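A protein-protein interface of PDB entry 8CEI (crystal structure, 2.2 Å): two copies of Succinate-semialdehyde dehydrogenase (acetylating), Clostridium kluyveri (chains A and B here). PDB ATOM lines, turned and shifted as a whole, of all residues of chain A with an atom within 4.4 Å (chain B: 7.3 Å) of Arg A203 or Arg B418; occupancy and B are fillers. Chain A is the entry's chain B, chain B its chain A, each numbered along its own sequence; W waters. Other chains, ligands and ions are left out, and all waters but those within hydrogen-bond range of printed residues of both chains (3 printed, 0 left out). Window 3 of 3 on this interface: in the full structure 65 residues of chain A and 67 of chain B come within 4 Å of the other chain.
The backbone NH of Gly A202 lies within hydrogen-bond range of the backbone carbonyl oxygen of Tyr B199, 2.8 Å away. NH1 of Arg A203 lies close to NE of Arg B418 (3.2 Å).
The backbone carbonyl oxygen of Lys B196 lies within hydrogen-bond range of the side-chain hydroxyl of Ser B200 (2.7 Å). OH of Tyr B199 lies within hydrogen-bond range of N of Gly B207 (3.3 Å). The backbone NH (N) of Ser B420 sits at hydrogen-bond distance from the side-chain hydroxyl (OH) of Tyr B199, at 2.6 Å. The backbone carbonyl oxygen (O) of Val B208 sits at hydrogen-bond distance from the side-chain amide nitrogen (ND2) of Asn B419, at 3.2 Å. O of Gly B417 lies within hydrogen-bond range of ND2 of Asn B419 (3.4 Å). The guanidinium group of Arg A203 lies within salt-bridge range of the side-chain carboxylate of Asp A184 (3.8 Å).
Ser A201 touches Tyr B199 (N to O, 3.6 Å). OG of Ser B200 touches N of Gly A202, at 3.5 Å. Tyr B199 touches Arg A203. Pro A204 touches Tyr B199. O of Asn B419 touches CG of Pro A204, at 3.5 Å. CB of Pro A204 touches CA of Ser B420 (3.8 Å).
Hydrophobic or aromatic side chains of chain B that line the printed part of chain A: Tyr B199. Of the 11 printed residues of chain A, 4 touch a printed residue of chain B. Printed residues of chain A that touch a printed residue of chain B: Ser A201, Gly A202, Arg A203 and Pro A204. Among the printed residues, no Asp or Glu carboxylate lies within 4 Å of a Lys or Arg side-chain nitrogen of the other chain.
Water W1 bridges the backbone carbonyl oxygen of Arg B418 and the backbone carbonyl oxygen of Gly A202. Water W3 lies within hydrogen-bond range of the backbone carbonyl oxygen of Ser A201 (2.9 Å), the backbone carbonyl oxygen of Glu A181 (3.1 Å) and the side-chain amino group of Lys B196 (3.2 Å). Water W2 lies within hydrogen-bond range of the backbone carbonyl oxygen (O) of Ser B415 (2.9 Å), the backbone carbonyl oxygen (O) of Asp A184 (2.9 Å) and the guanidinium group (NH1) of Arg A203 (3.0 Å).
Printed residues of chain B within 4 Å of Ser A201: Tyr B199 (3.6 Å). Printed residues of chain A within 4 Å of Tyr B199: Ser A201 (3.6 Å), Gly A202 (2.8 Å), Arg A203 (3.8 Å) and Pro A204 (3.9 Å). Of the printed residues of chain A, Ser B200 touches Gly A202. Gly B414 touches none of the printed residues of chain A. Printed residues of chain A within 4 Å of Asn B419: Pro A204 (3.5 Å). Of the printed residues of chain A, Ser B420 touches Pro A204. Ile B421 touches none of the printed residues of chain A. The nearest residue of chain A that does not touch Arg B418 is Pro A204 (4.1 Å). The nearest printed residue of chain A that does not touch Ser B420 is Ala A205 (6.0 Å).
1 position is printed for both chains. Of the 8 pairs that touch across the chains among the printed residues, none has its exchanged pair printed and touching as well.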
ATOM      1  N   MET A 180      19.212 -20.416  27.210  1.00  0.00           N
ATOM      2  CA  MET A 180      18.111 -19.818  27.957  1.00  0.00           C
ATOM      3  C   MET A 180      16.789 -19.974  27.216  1.00  0.00           C
ATOM      4  O   MET A 180      15.742 -20.184  27.840  1.00  0.00           O
ATOM      5  CB  MET A 180      18.406 -18.345  28.235  1.00  0.00           C
ATOM      6  CG  MET A 180      19.605 -18.115  29.144  1.00  0.00           C
ATOM      7  SD  MET A 180      19.943 -16.367  29.435  1.00  0.00           S
ATOM      8  CE  MET A 180      20.327 -15.822  27.774  1.00  0.00           C
ATOM      9  N   GLU A 181      16.814 -19.883  25.884  1.00  0.00           N
ATOM     10  CA  GLU A 181      15.584 -20.012  25.111  1.00  0.00           C
ATOM     11  C   GLU A 181      15.067 -21.445  25.102  1.00  0.00           C
ATOM     12  O   GLU A 181      13.852 -21.662  25.017  1.00  0.00           O
ATOM     13  CB  GLU A 181      15.810 -19.522  23.681  1.00  0.00           C
ATOM     14  CG  GLU A 181      16.147 -18.045  23.572  1.00  0.00           C
ATOM     15  CD  GLU A 181      16.575 -17.650  22.173  1.00  0.00           C
ATOM     16  OE1 GLU A 181      16.766 -18.553  21.332  1.00  0.00           O
ATOM     17  OE2 GLU A 181      16.719 -16.437  21.913  1.00  0.00           O
ATOM     18  N   SER A 182      15.963 -22.427  25.193  1.00  0.00           N
ATOM     19  CA  SER A 182      15.585 -23.833  25.111  1.00  0.00           C
ATOM     20  C   SER A 182      15.131 -24.408  26.447  1.00  0.00           C
ATOM     21  O   SER A 182      14.344 -25.361  26.465  1.00  0.00           O
ATOM     22  CB  SER A 182      16.755 -24.664  24.577  1.00  0.00           C
ATOM     23  OG  SER A 182      17.255 -24.128  23.365  1.00  0.00           O
ATOM     24  N   ALA A 183      15.610 -23.862  27.560  1.00  0.00           N
ATOM     25  CA  ALA A 183      15.233 -24.373  28.867  1.00  0.00           C
ATOM     26  C   ALA A 183      13.794 -23.983  29.199  1.00  0.00           C
ATOM     27  O   ALA A 183      13.164 -23.168  28.518  1.00  0.00           O
ATOM     28  CB  ALA A 183      16.184 -23.853  29.942  1.00  0.00           C
ATOM     29  N   ASP A 184      13.275 -24.577  30.271  1.00  0.00           N
ATOM     30  CA  ASP A 184      11.920 -24.298  30.726  1.00  0.00           C
ATOM     31  C   ASP A 184      11.846 -23.118  31.684  1.00  0.00           C
ATOM     32  O   ASP A 184      10.787 -22.489  31.791  1.00  0.00           O
ATOM     33  CB  ASP A 184      11.329 -25.538  31.402  1.00  0.00           C
ATOM     34  CG  ASP A 184      11.245 -26.723  30.464  1.00  0.00           C
ATOM     35  OD1 ASP A 184      10.590 -26.597  29.408  1.00  0.00           O
ATOM     36  OD2 ASP A 184      11.846 -27.773  30.774  1.00  0.00           O
ATOM     37  N   ALA A 198      18.059 -12.910  30.110  1.00  0.00           N
ATOM     38  CA  ALA A 198      17.191 -13.943  30.661  1.00  0.00           C
ATOM     39  C   ALA A 198      15.722 -13.598  30.455  1.00  0.00           C
ATOM     40  O   ALA A 198      14.919 -14.465  30.093  1.00  0.00           O
ATOM     41  CB  ALA A 198      17.491 -14.147  32.145  1.00  0.00           C
ATOM     42  N   SER A 201      14.334 -14.071  26.608  1.00  0.00           N
ATOM     43  CA  SER A 201      14.486 -15.393  26.018  1.00  0.00           C
ATOM     44  C   SER A 201      13.162 -16.059  25.673  1.00  0.00           C
ATOM     45  O   SER A 201      13.167 -17.177  25.150  1.00  0.00           O
ATOM     46  CB  SER A 201      15.275 -16.301  26.967  1.00  0.00           C
ATOM     47  OG  SER A 201      14.535 -16.560  28.148  1.00  0.00           O
ATOM     48  N   GLY A 202      12.033 -15.411  25.952  1.00  0.00           N
ATOM     49  CA  GLY A 202      10.742 -16.029  25.728  1.00  0.00           C
ATOM     50  C   GLY A 202      10.347 -17.068  26.751  1.00  0.00           C
ATOM     51  O   GLY A 202       9.350 -17.768  26.546  1.00  0.00           O
ATOM     52  N   ARG A 203      11.092 -17.189  27.845  1.00  0.00           N
ATOM     53  CA  ARG A 203      10.842 -18.158  28.897  1.00  0.00           C
ATOM     54  C   ARG A 203      10.749 -17.449  30.239  1.00  0.00           C
ATOM     55  O   ARG A 203      11.337 -16.378  30.420  1.00  0.00           O
ATOM     56  CB  ARG A 203      11.958 -19.211  28.952  1.00  0.00           C
ATOM     57  CG  ARG A 203      12.087 -20.059  27.698  1.00  0.00           C
ATOM     58  CD  ARG A 203      10.983 -21.097  27.615  1.00  0.00           C
ATOM     59  NE  ARG A 203      11.240 -22.075  26.566  1.00  0.00           N
ATOM     60  CZ  ARG A 203      10.587 -23.221  26.432  1.00  0.00           C
ATOM     61  NH1 ARG A 203       9.631 -23.575  27.276  1.00  0.00           N
ATOM     62  NH2 ARG A 203      10.903 -24.035  25.429  1.00  0.00           N
ATOM     63  N   PRO A 204      10.015 -18.018  31.196  1.00  0.00           N
ATOM     64  CA  PRO A 204       9.991 -17.434  32.545  1.00  0.00           C
ATOM     65  C   PRO A 204      11.383 -17.442  33.158  1.00  0.00           C
ATOM     66  O   PRO A 204      12.066 -18.469  33.181  1.00  0.00           O
ATOM     67  CB  PRO A 204       9.022 -18.342  33.311  1.00  0.00           C
ATOM     68  CG  PRO A 204       8.980 -19.618  32.525  1.00  0.00           C
ATOM     69  CD  PRO A 204       9.157 -19.211  31.094  1.00  0.00           C
ATOM     70  N   ALA A 205      11.806 -16.280  33.652  1.00  0.00           N
ATOM     71  CA  ALA A 205      13.169 -16.089  34.124  1.00  0.00           C
ATOM     72  C   ALA A 205      13.171 -15.544  35.544  1.00  0.00           C
ATOM     73  O   ALA A 205      12.238 -14.857  35.969  1.00  0.00           O
ATOM     74  CB  ALA A 205      13.950 -15.137  33.207  1.00  0.00           C
ATOM     75  N   VAL B 195       2.117 -13.943  23.985  1.00  0.00           N
ATOM     76  CA  VAL B 195       2.753 -14.317  25.244  1.00  0.00           C
ATOM     77  C   VAL B 195       4.264 -14.417  25.072  1.00  0.00           C
ATOM     78  O   VAL B 195       5.030 -13.979  25.938  1.00  0.00           O
ATOM     79  CB  VAL B 195       2.150 -15.630  25.774  1.00  0.00           C
ATOM     80  CG1 VAL B 195       2.823 -16.042  27.075  1.00  0.00           C
ATOM     81  CG2 VAL B 195       0.649 -15.482  25.969  1.00  0.00           C
ATOM     82  N   LYS B 196       4.716 -14.992  23.954  1.00  0.00           N
ATOM     83  CA  LYS B 196       6.150 -15.104  23.704  1.00  0.00           C
ATOM     84  C   LYS B 196       6.796 -13.729  23.578  1.00  0.00           C
ATOM     85  O   LYS B 196       7.937 -13.528  24.012  1.00  0.00           O
ATOM     86  CB  LYS B 196       6.401 -15.933  22.446  1.00  0.00           C
ATOM     87  CG  LYS B 196       7.871 -16.153  22.127  1.00  0.00           C
ATOM     88  CD  LYS B 196       8.045 -16.924  20.827  1.00  0.00           C
ATOM     89  CE  LYS B 196       9.515 -17.169  20.522  1.00  0.00           C
ATOM     90  NZ  LYS B 196      10.159 -18.018  21.560  1.00  0.00           N
ATOM     91  N   TYR B 199       7.376 -12.361  27.147  1.00  0.00           N
ATOM     92  CA  TYR B 199       8.551 -12.932  27.794  1.00  0.00           C
ATOM     93  C   TYR B 199       9.835 -12.694  27.009  1.00  0.00           C
ATOM     94  O   TYR B 199      10.870 -13.277  27.350  1.00  0.00           O
ATOM     95  CB  TYR B 199       8.347 -14.432  28.030  1.00  0.00           C
ATOM     96  CG  TYR B 199       7.390 -14.735  29.159  1.00  0.00           C
ATOM     97  CD1 TYR B 199       7.844 -14.862  30.466  1.00  0.00           C
ATOM     98  CD2 TYR B 199       6.030 -14.886  28.920  1.00  0.00           C
ATOM     99  CE1 TYR B 199       6.971 -15.134  31.504  1.00  0.00           C
ATOM    100  CE2 TYR B 199       5.149 -15.160  29.950  1.00  0.00           C
ATOM    101  CZ  TYR B 199       5.625 -15.283  31.240  1.00  0.00           C
ATOM    102  OH  TYR B 199       4.752 -15.553  32.268  1.00  0.00           O
ATOM    103  N   SER B 200       9.791 -11.852  25.975  1.00  0.00           N
ATOM    104  CA  SER B 200      10.979 -11.463  25.225  1.00  0.00           C
ATOM    105  C   SER B 200      11.268  -9.971  25.337  1.00  0.00           C
ATOM    106  O   SER B 200      12.141  -9.465  24.623  1.00  0.00           O
ATOM    107  CB  SER B 200      10.831 -11.853  23.752  1.00  0.00           C
ATOM    108  OG  SER B 200      10.598 -13.242  23.607  1.00  0.00           O
ATOM    109  N   ALA B 205       7.101 -10.644  33.093  1.00  0.00           N
ATOM    110  CA  ALA B 205       5.859 -10.783  32.350  1.00  0.00           C
ATOM    111  C   ALA B 205       4.982 -11.859  32.974  1.00  0.00           C
ATOM    112  O   ALA B 205       5.458 -12.757  33.675  1.00  0.00           O
ATOM    113  CB  ALA B 205       6.123 -11.116  30.875  1.00  0.00           C
ATOM    114  N   TYR B 206       3.682 -11.749  32.706  1.00  0.00           N
ATOM    115  CA  TYR B 206       2.696 -12.752  33.086  1.00  0.00           C
ATOM    116  C   TYR B 206       1.846 -13.060  31.865  1.00  0.00           C
ATOM    117  O   TYR B 206       1.256 -12.150  31.273  1.00  0.00           O
ATOM    118  CB  TYR B 206       1.821 -12.268  34.246  1.00  0.00           C
ATOM    119  CG  TYR B 206       2.577 -12.079  35.539  1.00  0.00           C
ATOM    120  CD1 TYR B 206       2.703 -13.119  36.450  1.00  0.00           C
ATOM    121  CD2 TYR B 206       3.170 -10.862  35.847  1.00  0.00           C
ATOM    122  CE1 TYR B 206       3.396 -12.952  37.634  1.00  0.00           C
ATOM    123  CE2 TYR B 206       3.867 -10.687  37.029  1.00  0.00           C
ATOM    124  CZ  TYR B 206       3.975 -11.734  37.919  1.00  0.00           C
ATOM    125  OH  TYR B 206       4.666 -11.565  39.096  1.00  0.00           O
ATOM    126  N   GLY B 207       1.789 -14.331  31.484  1.00  0.00           N
ATOM    127  CA  GLY B 207       1.046 -14.706  30.299  1.00  0.00           C
ATOM    128  C   GLY B 207       0.089 -15.857  30.511  1.00  0.00           C
ATOM    129  O   GLY B 207      -0.194 -16.249  31.646  1.00  0.00           O
ATOM    130  N   VAL B 208      -0.423 -16.401  29.407  1.00  0.00           N
ATOM    131  CA  VAL B 208      -1.295 -17.564  29.421  1.00  0.00           C
ATOM    132  C   VAL B 208      -0.755 -18.576  28.420  1.00  0.00           C
ATOM    133  O   VAL B 208       0.118 -18.277  27.604  1.00  0.00           O
ATOM    134  CB  VAL B 208      -2.760 -17.209  29.090  1.00  0.00           C
ATOM    135  CG1 VAL B 208      -3.342 -16.298  30.154  1.00  0.00           C
ATOM    136  CG2 VAL B 208      -2.851 -16.562  27.717  1.00  0.00           C
ATOM    137  N   GLY B 209      -1.287 -19.790  28.498  1.00  0.00           N
ATOM    138  CA  GLY B 209      -0.956 -20.825  27.551  1.00  0.00           C
ATOM    139  C   GLY B 209      -2.183 -21.282  26.795  1.00  0.00           C
ATOM    140  O   GLY B 209      -3.319 -20.962  27.161  1.00  0.00           O
ATOM    141  N   PRO B 210      -1.981 -22.035  25.716  1.00  0.00           N
ATOM    142  CA  PRO B 210      -3.127 -22.559  24.967  1.00  0.00           C
ATOM    143  C   PRO B 210      -3.934 -23.526  25.819  1.00  0.00           C
ATOM    144  O   PRO B 210      -3.382 -24.361  26.536  1.00  0.00           O
ATOM    145  CB  PRO B 210      -2.478 -23.264  23.770  1.00  0.00           C
ATOM    146  CG  PRO B 210      -1.104 -23.612  24.242  1.00  0.00           C
ATOM    147  CD  PRO B 210      -0.696 -22.489  25.156  1.00  0.00           C
ATOM    148  N   ALA B 362      -0.933 -28.358  27.239  1.00  0.00           N
ATOM    149  CA  ALA B 362      -0.325 -28.767  28.498  1.00  0.00           C
ATOM    150  C   ALA B 362      -0.092 -27.561  29.401  1.00  0.00           C
ATOM    151  O   ALA B 362       0.347 -26.500  28.949  1.00  0.00           O
ATOM    152  CB  ALA B 362       0.994 -29.495  28.240  1.00  0.00           C
ATOM    153  N   CYS B 413      -0.507 -20.673  32.933  1.00  0.00           N
ATOM    154  CA  CYS B 413      -0.378 -22.101  32.659  1.00  0.00           C
ATOM    155  C   CYS B 413       0.998 -22.650  33.021  1.00  0.00           C
ATOM    156  O   CYS B 413       1.387 -23.711  32.522  1.00  0.00           O
ATOM    157  CB  CYS B 413      -0.695 -22.387  31.191  1.00  0.00           C
ATOM    158  SG  CYS B 413      -2.376 -21.934  30.716  1.00  0.00           S
ATOM    159  N   GLY B 414       1.742 -21.953  33.876  1.00  0.00           N
ATOM    160  CA  GLY B 414       2.995 -22.488  34.373  1.00  0.00           C
ATOM    161  C   GLY B 414       4.070 -22.627  33.304  1.00  0.00           C
ATOM    162  O   GLY B 414       3.997 -22.056  32.212  1.00  0.00           O
ATOM    163  N   SER B 415       5.089 -23.421  33.646  1.00  0.00           N
ATOM    164  CA  SER B 415       6.225 -23.605  32.747  1.00  0.00           C
ATOM    165  C   SER B 415       5.834 -24.369  31.488  1.00  0.00           C
ATOM    166  O   SER B 415       6.475 -24.203  30.443  1.00  0.00           O
ATOM    167  CB  SER B 415       7.359 -24.328  33.475  1.00  0.00           C
ATOM    168  OG  SER B 415       6.969 -25.637  33.853  1.00  0.00           O
ATOM    169  N   TRP B 416       4.800 -25.212  31.567  1.00  0.00           N
ATOM    170  CA  TRP B 416       4.341 -25.934  30.384  1.00  0.00           C
ATOM    171  C   TRP B 416       3.895 -24.967  29.295  1.00  0.00           C
ATOM    172  O   TRP B 416       4.312 -25.079  28.137  1.00  0.00           O
ATOM    173  CB  TRP B 416       3.202 -26.882  30.753  1.00  0.00           C
ATOM    174  CG  TRP B 416       3.534 -27.869  31.826  1.00  0.00           C
ATOM    175  CD1 TRP B 416       4.228 -29.035  31.682  1.00  0.00           C
ATOM    176  CD2 TRP B 416       3.164 -27.790  33.209  1.00  0.00           C
ATOM    177  NE1 TRP B 416       4.323 -29.682  32.891  1.00  0.00           N
ATOM    178  CE2 TRP B 416       3.677 -28.940  33.843  1.00  0.00           C
ATOM    179  CE3 TRP B 416       2.453 -26.857  33.971  1.00  0.00           C
ATOM    180  CZ2 TRP B 416       3.501 -29.180  35.204  1.00  0.00           C
ATOM    181  CZ3 TRP B 416       2.279 -27.099  35.323  1.00  0.00           C
ATOM    182  CH2 TRP B 416       2.802 -28.252  35.925  1.00  0.00           C
ATOM    183  N   GLY B 417       3.041 -24.009  29.651  1.00  0.00           N
ATOM    184  CA  GLY B 417       2.607 -22.974  28.738  1.00  0.00           C
ATOM    185  C   GLY B 417       3.542 -21.794  28.629  1.00  0.00           C
ATOM    186  O   GLY B 417       3.157 -20.760  28.075  1.00  0.00           O
ATOM    187  N   ARG B 418       4.763 -21.924  29.152  1.00  0.00           N
ATOM    188  CA  ARG B 418       5.771 -20.865  29.123  1.00  0.00           C
ATOM    189  C   ARG B 418       5.259 -19.597  29.806  1.00  0.00           C
ATOM    190  O   ARG B 418       5.338 -18.490  29.267  1.00  0.00           O
ATOM    191  CB  ARG B 418       6.230 -20.585  27.689  1.00  0.00           C
ATOM    192  CG  ARG B 418       6.652 -21.842  26.945  1.00  0.00           C
ATOM    193  CD  ARG B 418       7.351 -21.529  25.637  1.00  0.00           C
ATOM    194  NE  ARG B 418       7.645 -22.747  24.890  1.00  0.00           N
ATOM    195  CZ  ARG B 418       8.403 -22.797  23.803  1.00  0.00           C
ATOM    196  NH1 ARG B 418       8.984 -21.713  23.314  1.00  0.00           N
ATOM    197  NH2 ARG B 418       8.586 -23.965  23.194  1.00  0.00           N
ATOM    198  N   ASN B 419       4.729 -19.773  31.014  1.00  0.00           N
ATOM    199  CA  ASN B 419       4.285 -18.676  31.858  1.00  0.00           C
ATOM    200  C   ASN B 419       5.060 -18.700  33.170  1.00  0.00           C
ATOM    201  O   ASN B 419       5.622 -19.726  33.564  1.00  0.00           O
ATOM    202  CB  ASN B 419       2.778 -18.751  32.137  1.00  0.00           C
ATOM    203  CG  ASN B 419       1.950 -18.799  30.867  1.00  0.00           C
ATOM    204  OD1 ASN B 419       0.989 -19.560  30.770  1.00  0.00           O
ATOM    205  ND2 ASN B 419       2.322 -17.986  29.885  1.00  0.00           N
ATOM    206  N   SER B 420       5.080 -17.551  33.848  1.00  0.00           N
ATOM    207  CA  SER B 420       5.824 -17.433  35.099  1.00  0.00           C
ATOM    208  C   SER B 420       5.127 -18.135  36.259  1.00  0.00           C
ATOM    209  O   SER B 420       5.802 -18.669  37.146  1.00  0.00           O
ATOM    210  CB  SER B 420       6.043 -15.960  35.444  1.00  0.00           C
ATOM    211  OG  SER B 420       4.805 -15.293  35.610  1.00  0.00           O
ATOM    212  N   ILE B 421       3.795 -18.139  36.278  1.00  0.00           N
ATOM    213  CA  ILE B 421       3.032 -18.732  37.368  1.00  0.00           C
ATOM    214  C   ILE B 421       2.105 -19.799  36.806  1.00  0.00           C
ATOM    215  O   ILE B 421       1.704 -19.756  35.639  1.00  0.00           O
ATOM    216  CB  ILE B 421       2.223 -17.679  38.158  1.00  0.00           C
ATOM    217  CG1 ILE B 421       1.168 -17.025  37.259  1.00  0.00           C
ATOM    218  CG2 ILE B 421       3.147 -16.632  38.767  1.00  0.00           C
ATOM    219  CD1 ILE B 421       0.297 -16.012  37.969  1.00  0.00           C
HETATM  220  O   HOH W   1       6.176 -17.397  26.897  1.00  0.00           O
HETATM  221  O   HOH W   2       8.615 -22.338  29.832  1.00  0.00           O
HETATM  222  O   HOH W   3      12.090 -19.435  23.711  1.00  0.00           O
